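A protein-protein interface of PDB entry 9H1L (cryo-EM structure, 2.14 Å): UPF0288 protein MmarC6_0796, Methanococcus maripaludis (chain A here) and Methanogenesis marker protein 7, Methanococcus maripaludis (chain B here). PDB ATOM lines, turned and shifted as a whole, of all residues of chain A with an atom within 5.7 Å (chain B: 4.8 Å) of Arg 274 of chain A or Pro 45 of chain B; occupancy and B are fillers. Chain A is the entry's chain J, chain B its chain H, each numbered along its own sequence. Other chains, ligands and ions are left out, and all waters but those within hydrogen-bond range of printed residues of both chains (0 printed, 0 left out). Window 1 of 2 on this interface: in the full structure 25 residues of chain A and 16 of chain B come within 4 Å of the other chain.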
ATOM      1  N   ASN A 229      -0.322 -20.898   8.152  1.00  0.00           N
ATOM      2  CA  ASN A 229       0.116 -21.259   9.490  1.00  0.00           C
ATOM      3  C   ASN A 229       0.446 -22.738   9.626  1.00  0.00           C
ATOM      4  O   ASN A 229       0.921 -23.153  10.687  1.00  0.00           O
ATOM      5  CB  ASN A 229      -0.951 -20.872  10.515  1.00  0.00           C
ATOM      6  CG  ASN A 229      -1.007 -19.379  10.761  1.00  0.00           C
ATOM      7  OD1 ASN A 229      -0.004 -18.678  10.623  1.00  0.00           O
ATOM      8  ND2 ASN A 229      -2.181 -18.883  11.128  1.00  0.00           N
ATOM      9  N   THR A 230       0.205 -23.540   8.588  1.00  0.00           N
ATOM     10  CA  THR A 230       0.428 -24.979   8.653  1.00  0.00           C
ATOM     11  C   THR A 230       1.433 -25.506   7.640  1.00  0.00           C
ATOM     12  O   THR A 230       1.993 -26.581   7.861  1.00  0.00           O
ATOM     13  CB  THR A 230      -0.892 -25.737   8.465  1.00  0.00           C
ATOM     14  OG1 THR A 230      -1.357 -25.565   7.121  1.00  0.00           O
ATOM     15  CG2 THR A 230      -1.945 -25.235   9.435  1.00  0.00           C
ATOM     16  N   ASP A 249      -0.135 -39.774   7.283  1.00  0.00           N
ATOM     17  CA  ASP A 249      -0.253 -38.565   8.086  1.00  0.00           C
ATOM     18  C   ASP A 249       0.739 -37.500   7.636  1.00  0.00           C
ATOM     19  O   ASP A 249       1.915 -37.789   7.398  1.00  0.00           O
ATOM     20  CB  ASP A 249      -0.032 -38.897   9.561  1.00  0.00           C
ATOM     21  CG  ASP A 249      -1.319 -39.236  10.278  1.00  0.00           C
ATOM     22  OD1 ASP A 249      -2.201 -39.864   9.656  1.00  0.00           O
ATOM     23  OD2 ASP A 249      -1.451 -38.875  11.466  1.00  0.00           O
ATOM     24  N   ARG A 250       0.253 -36.263   7.518  1.00  0.00           N
ATOM     25  CA  ARG A 250       1.094 -35.114   7.194  1.00  0.00           C
ATOM     26  C   ARG A 250       1.600 -34.518   8.505  1.00  0.00           C
ATOM     27  O   ARG A 250       1.107 -33.503   9.003  1.00  0.00           O
ATOM     28  CB  ARG A 250       0.317 -34.097   6.368  1.00  0.00           C
ATOM     29  CG  ARG A 250      -0.180 -34.632   5.038  1.00  0.00           C
ATOM     30  CD  ARG A 250      -1.057 -33.617   4.328  1.00  0.00           C
ATOM     31  NE  ARG A 250      -2.385 -33.534   4.923  1.00  0.00           N
ATOM     32  CZ  ARG A 250      -3.309 -32.653   4.569  1.00  0.00           C
ATOM     33  NH1 ARG A 250      -3.082 -31.755   3.625  1.00  0.00           N
ATOM     34  NH2 ARG A 250      -4.491 -32.673   5.177  1.00  0.00           N
ATOM     35  N   ASP A 251       2.608 -35.174   9.071  1.00  0.00           N
ATOM     36  CA  ASP A 251       3.111 -34.821  10.391  1.00  0.00           C
ATOM     37  C   ASP A 251       3.978 -33.566  10.313  1.00  0.00           C
ATOM     38  O   ASP A 251       4.054 -32.885   9.287  1.00  0.00           O
ATOM     39  CB  ASP A 251       3.882 -35.991  10.993  1.00  0.00           C
ATOM     40  CG  ASP A 251       3.088 -37.278  10.981  1.00  0.00           C
ATOM     41  OD1 ASP A 251       1.963 -37.288  11.522  1.00  0.00           O
ATOM     42  OD2 ASP A 251       3.589 -38.282  10.432  1.00  0.00           O
ATOM     43  N   TYR A 270       5.058 -29.270   5.718  1.00  0.00           N
ATOM     44  CA  TYR A 270       4.056 -29.008   6.744  1.00  0.00           C
ATOM     45  C   TYR A 270       4.719 -28.654   8.068  1.00  0.00           C
ATOM     46  O   TYR A 270       5.595 -29.380   8.546  1.00  0.00           O
ATOM     47  CB  TYR A 270       3.142 -30.220   6.919  1.00  0.00           C
ATOM     48  CG  TYR A 270       1.967 -30.227   5.971  1.00  0.00           C
ATOM     49  CD1 TYR A 270       2.110 -30.658   4.660  1.00  0.00           C
ATOM     50  CD2 TYR A 270       0.717 -29.791   6.383  1.00  0.00           C
ATOM     51  CE1 TYR A 270       1.040 -30.661   3.790  1.00  0.00           C
ATOM     52  CE2 TYR A 270      -0.358 -29.790   5.520  1.00  0.00           C
ATOM     53  CZ  TYR A 270      -0.190 -30.226   4.224  1.00  0.00           C
ATOM     54  OH  TYR A 270      -1.261 -30.227   3.362  1.00  0.00           O
ATOM     55  N   GLU A 272       2.786 -28.249  10.814  1.00  0.00           N
ATOM     56  CA  GLU A 272       1.852 -28.689  11.841  1.00  0.00           C
ATOM     57  C   GLU A 272       1.437 -30.125  11.561  1.00  0.00           C
ATOM     58  O   GLU A 272       1.421 -30.569  10.411  1.00  0.00           O
ATOM     59  CB  GLU A 272       0.612 -27.790  11.900  1.00  0.00           C
ATOM     60  CG  GLU A 272       0.904 -26.350  12.279  1.00  0.00           C
ATOM     61  CD  GLU A 272       0.655 -26.073  13.747  1.00  0.00           C
ATOM     62  OE1 GLU A 272      -0.150 -26.803  14.362  1.00  0.00           O
ATOM     63  OE2 GLU A 272       1.262 -25.122  14.282  1.00  0.00           O
ATOM     64  N   SER A 273       1.098 -30.846  12.625  1.00  0.00           N
ATOM     65  CA  SER A 273       0.669 -32.238  12.515  1.00  0.00           C
ATOM     66  C   SER A 273      -0.787 -32.260  12.069  1.00  0.00           C
ATOM     67  O   SER A 273      -1.690 -31.915  12.835  1.00  0.00           O
ATOM     68  CB  SER A 273       0.854 -32.966  13.842  1.00  0.00           C
ATOM     69  OG  SER A 273       2.224 -33.054  14.190  1.00  0.00           O
ATOM     70  N   ARG A 274      -1.019 -32.661  10.826  1.00  0.00           N
ATOM     71  CA  ARG A 274      -2.352 -32.707  10.244  1.00  0.00           C
ATOM     72  C   ARG A 274      -2.700 -34.129   9.830  1.00  0.00           C
ATOM     73  O   ARG A 274      -1.873 -35.043   9.876  1.00  0.00           O
ATOM     74  CB  ARG A 274      -2.451 -31.758   9.045  1.00  0.00           C
ATOM     75  CG  ARG A 274      -2.161 -30.310   9.391  1.00  0.00           C
ATOM     76  CD  ARG A 274      -3.447 -29.516   9.516  1.00  0.00           C
ATOM     77  NE  ARG A 274      -3.255 -28.251  10.215  1.00  0.00           N
ATOM     78  CZ  ARG A 274      -3.242 -28.120  11.534  1.00  0.00           C
ATOM     79  NH1 ARG A 274      -3.403 -29.161  12.334  1.00  0.00           N
ATOM     80  NH2 ARG A 274      -3.064 -26.913  12.064  1.00  0.00           N
ATOM     81  N   ALA A 275      -3.953 -34.307   9.423  1.00  0.00           N
ATOM     82  CA  ALA A 275      -4.456 -35.616   9.044  1.00  0.00           C
ATOM     83  C   ALA A 275      -4.010 -35.981   7.630  1.00  0.00           C
ATOM     84  O   ALA A 275      -3.547 -35.144   6.854  1.00  0.00           O
ATOM     85  CB  ALA A 275      -5.979 -35.653   9.147  1.00  0.00           C
ATOM     86  N   SER A 276      -4.158 -37.261   7.304  1.00  0.00           N
ATOM     87  CA  SER A 276      -3.830 -37.743   5.972  1.00  0.00           C
ATOM     88  C   SER A 276      -4.789 -37.168   4.936  1.00  0.00           C
ATOM     89  O   SER A 276      -5.943 -36.852   5.232  1.00  0.00           O
ATOM     90  CB  SER A 276      -3.878 -39.271   5.934  1.00  0.00           C
ATOM     91  OG  SER A 276      -3.923 -39.744   4.603  1.00  0.00           O
ATOM     92  N   MET B   1      -9.826 -27.097  18.884  1.00  0.00           N
ATOM     93  CA  MET B   1      -8.855 -26.556  17.940  1.00  0.00           C
ATOM     94  C   MET B   1      -9.475 -26.482  16.551  1.00  0.00           C
ATOM     95  O   MET B   1      -9.026 -25.714  15.702  1.00  0.00           O
ATOM     96  CB  MET B   1      -7.567 -27.404  17.958  1.00  0.00           C
ATOM     97  CG  MET B   1      -7.447 -28.564  16.952  1.00  0.00           C
ATOM     98  SD  MET B   1      -6.921 -28.172  15.262  1.00  0.00           S
ATOM     99  CE  MET B   1      -5.357 -27.356  15.573  1.00  0.00           C
ATOM    100  N   TYR B   2     -10.520 -27.278  16.328  1.00  0.00           N
ATOM    101  CA  TYR B   2     -11.185 -27.358  15.029  1.00  0.00           C
ATOM    102  C   TYR B   2     -12.473 -26.547  15.105  1.00  0.00           C
ATOM    103  O   TYR B   2     -13.528 -27.050  15.494  1.00  0.00           O
ATOM    104  CB  TYR B   2     -11.451 -28.807  14.646  1.00  0.00           C
ATOM    105  CG  TYR B   2     -10.285 -29.475  13.956  1.00  0.00           C
ATOM    106  CD1 TYR B   2      -9.743 -28.941  12.795  1.00  0.00           C
ATOM    107  CD2 TYR B   2      -9.716 -30.630  14.474  1.00  0.00           C
ATOM    108  CE1 TYR B   2      -8.673 -29.545  12.164  1.00  0.00           C
ATOM    109  CE2 TYR B   2      -8.644 -31.238  13.852  1.00  0.00           C
ATOM    110  CZ  TYR B   2      -8.127 -30.692  12.697  1.00  0.00           C
ATOM    111  OH  TYR B   2      -7.061 -31.298  12.074  1.00  0.00           O
ATOM    112  N   VAL B  24      -4.702 -26.851   4.023  1.00  0.00           N
ATOM    113  CA  VAL B  24      -4.497 -26.391   5.397  1.00  0.00           C
ATOM    114  C   VAL B  24      -5.004 -27.381   6.431  1.00  0.00           C
ATOM    115  O   VAL B  24      -4.951 -27.086   7.632  1.00  0.00           O
ATOM    116  CB  VAL B  24      -5.163 -25.022   5.650  1.00  0.00           C
ATOM    117  CG1 VAL B  24      -4.667 -24.000   4.646  1.00  0.00           C
ATOM    118  CG2 VAL B  24      -6.675 -25.140   5.595  1.00  0.00           C
ATOM    119  N   GLY B  25      -5.489 -28.543   6.009  1.00  0.00           N
ATOM    120  CA  GLY B  25      -5.936 -29.564   6.930  1.00  0.00           C
ATOM    121  C   GLY B  25      -7.396 -29.505   7.318  1.00  0.00           C
ATOM    122  O   GLY B  25      -7.811 -30.258   8.205  1.00  0.00           O
ATOM    123  N   GLY B  26      -8.186 -28.639   6.690  1.00  0.00           N
ATOM    124  CA  GLY B  26      -9.598 -28.579   6.996  1.00  0.00           C
ATOM    125  C   GLY B  26     -10.367 -29.745   6.406  1.00  0.00           C
ATOM    126  O   GLY B  26      -9.909 -30.447   5.506  1.00  0.00           O
ATOM    127  N   ALA B  43     -14.779 -27.617   8.988  1.00  0.00           N
ATOM    128  CA  ALA B  43     -14.036 -27.603  10.244  1.00  0.00           C
ATOM    129  C   ALA B  43     -12.564 -27.380   9.921  1.00  0.00           C
ATOM    130  O   ALA B  43     -11.912 -28.257   9.346  1.00  0.00           O
ATOM    131  CB  ALA B  43     -14.239 -28.901  11.016  1.00  0.00           C
ATOM    132  N   ILE B  44     -12.043 -26.217  10.285  1.00  0.00           N
ATOM    133  CA  ILE B  44     -10.657 -25.860   9.998  1.00  0.00           C
ATOM    134  C   ILE B  44      -9.945 -25.645  11.327  1.00  0.00           C
ATOM    135  O   ILE B  44     -10.593 -25.394  12.358  1.00  0.00           O
ATOM    136  CB  ILE B  44     -10.561 -24.617   9.081  1.00  0.00           C
ATOM    137  CG1 ILE B  44     -10.918 -23.338   9.830  1.00  0.00           C
ATOM    138  CG2 ILE B  44     -11.433 -24.768   7.859  1.00  0.00           C
ATOM    139  CD1 ILE B  44     -10.123 -22.165   9.343  1.00  0.00           C
ATOM    140  N   PRO B  45      -8.614 -25.780  11.353  1.00  0.00           N
ATOM    141  CA  PRO B  45      -7.869 -25.481  12.582  1.00  0.00           C
ATOM    142  C   PRO B  45      -7.994 -24.018  12.983  1.00  0.00           C
ATOM    143  O   PRO B  45      -8.145 -23.129  12.142  1.00  0.00           O
ATOM    144  CB  PRO B  45      -6.424 -25.835  12.218  1.00  0.00           C
ATOM    145  CG  PRO B  45      -6.543 -26.817  11.123  1.00  0.00           C
ATOM    146  CD  PRO B  45      -7.755 -26.431  10.345  1.00  0.00           C
ATOM    147  N   GLN B  46      -7.927 -23.780  14.297  1.00  0.00           N
ATOM    148  CA  GLN B  46      -8.164 -22.451  14.846  1.00  0.00           C
ATOM    149  C   GLN B  46      -7.070 -21.453  14.483  1.00  0.00           C
ATOM    150  O   GLN B  46      -7.316 -20.243  14.533  1.00  0.00           O
ATOM    151  CB  GLN B  46      -8.306 -22.525  16.365  1.00  0.00           C
ATOM    152  CG  GLN B  46      -9.643 -22.024  16.886  1.00  0.00           C
ATOM    153  CD  GLN B  46      -9.740 -22.093  18.395  1.00  0.00           C
ATOM    154  OE1 GLN B  46      -9.097 -22.927  19.033  1.00  0.00           O
ATOM    155  NE2 GLN B  46     -10.549 -21.213  18.977  1.00  0.00           N
ATOM    156  N   ASN B  47      -5.879 -21.921  14.119  1.00  0.00           N
ATOM    157  CA  ASN B  47      -4.810 -21.016  13.720  1.00  0.00           C
ATOM    158  C   ASN B  47      -4.938 -20.556  12.274  1.00  0.00           C
ATOM    159  O   ASN B  47      -4.123 -19.742  11.827  1.00  0.00           O
ATOM    160  CB  ASN B  47      -3.448 -21.681  13.934  1.00  0.00           C
ATOM    161  CG  ASN B  47      -3.421 -23.120  13.470  1.00  0.00           C
ATOM    162  OD1 ASN B  47      -4.062 -23.988  14.059  1.00  0.00           O
ATOM    163  ND2 ASN B  47      -2.673 -23.382  12.406  1.00  0.00           N
ATOM    164  N   GLU B  48      -5.930 -21.052  11.539  1.00  0.00           N
ATOM    165  CA  GLU B  48      -6.160 -20.656  10.159  1.00  0.00           C
ATOM    166  C   GLU B  48      -7.461 -19.887   9.975  1.00  0.00           C
ATOM    167  O   GLU B  48      -7.927 -19.751   8.838  1.00  0.00           O
ATOM    168  CB  GLU B  48      -6.150 -21.885   9.249  1.00  0.00           C
ATOM    169  CG  GLU B  48      -4.806 -22.587   9.166  1.00  0.00           C
ATOM    170  CD  GLU B  48      -3.929 -22.058   8.048  1.00  0.00           C
ATOM    171  OE1 GLU B  48      -3.920 -20.836   7.804  1.00  0.00           O
ATOM    172  OE2 GLU B  48      -3.243 -22.874   7.400  1.00  0.00           O
ATOM    173  N   ILE B  49      -8.051 -19.379  11.061  1.00  0.00           N
ATOM    174  CA  ILE B  49      -9.325 -18.664  10.986  1.00  0.00           C
ATOM    175  C   ILE B  49      -9.187 -17.403  10.138  1.00  0.00           C
ATOM    176  O   ILE B  49      -9.978 -17.156   9.219  1.00  0.00           O
ATOM    177  CB  ILE B  49      -9.832 -18.336  12.403  1.00  0.00           C
ATOM    178  CG1 ILE B  49     -10.486 -19.554  13.063  1.00  0.00           C
ATOM    179  CG2 ILE B  49     -10.828 -17.185  12.376  1.00  0.00           C
ATOM    180  CD1 ILE B  49     -11.448 -20.298  12.176  1.00  0.00           C
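The side-chain carboxylate (OE2) of Glu 48 of chain B is in hydrogen-bond range of the side-chain hydroxyl (OG1) of Thr 230 of chain A, at 3.3 Å.
NE of Arg 274 of chain A sits at hydrogen-bond distance from O of Val 24 of chain B (3.3 Å).
The backbone carbonyl oxygen of Asn 47 of chain B sits close to the side-chain amide nitrogen of Asn 229 of chain A, 2.2 Å away.
The backbone carbonyl oxygen (O) of Thr 230 of chain A sits at hydrogen-bond distance from the backbone NH (N) of Glu 272 of chain A (3.5 Å).
The backbone carbonyl oxygen (O) of Arg 250 of chain A sits at hydrogen-bond distance from the backbone NH (N) of Arg 274 of chain A (2.9 Å).
The backbone carbonyl oxygen (O) of Ala 275 of chain A sits at hydrogen-bond distance from the guanidinium group (NE) of Arg 250 of chain A, 2.8 Å away.
The guanidinium group (NH2) of Arg 274 of chain A lies within salt-bridge range of the side-chain carboxylate (OE1) of Glu 272 of chain A (3.7 Å).
Asn 229 of chain A touches Glu 48 of chain B.
Val 24 of chain B touches Thr 230 of chain A (CA to OG1, 3.7 Å).
ND2 of Asn 47 of chain B touches CG2 of Thr 230 of chain A, 3.6 Å away.
Arg 250 of chain A touches Gly 25 of chain B (NH2 to CA, 3.9 Å).
Arg 274 of chain A touches Gly 25 of chain B.
Pro 45 of chain B touches Arg 274 of chain A (CB to NH2, 3.5 Å).
Arg 274 of chain A touches Asn 47 of chain B (NH2 to ND2, 3.6 Å).
Of the printed residues of chain B, Asn 229 of chain A touches Asn 47 (2.2 Å) and Glu 48 (3.6 Å).
Of the printed residues of chain B, Thr 230 of chain A touches Val 24, Asn 47 and Glu 48.
Arg 274 of chain A touches just these residues of chain B: Val 24, Gly 25, Pro 45 and Asn 47.
Met 1 of chain B touches none of the printed residues of chain A.
Of the printed residues of chain A, Gly 25 of chain B touches Arg 250 and Arg 274.
Pro 45 of chain B touches one residue of chain A.
The nearest residue of chain A that does not touch Pro 45 of chain B is Thr 230 of chain A (5.1 Å).
Of the 12 printed residues of chain B, 5 touch a printed residue of chain A.
Along chain A the printed residues that touch a printed residue of chain B span positions 229 to 274.
Among the printed residues, 10 pairs touch across the chains.
Among the printed residues, no Asp or Glu carboxylate lies within 4 Å of a Lys or Arg side-chain nitrogen of the other chain.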
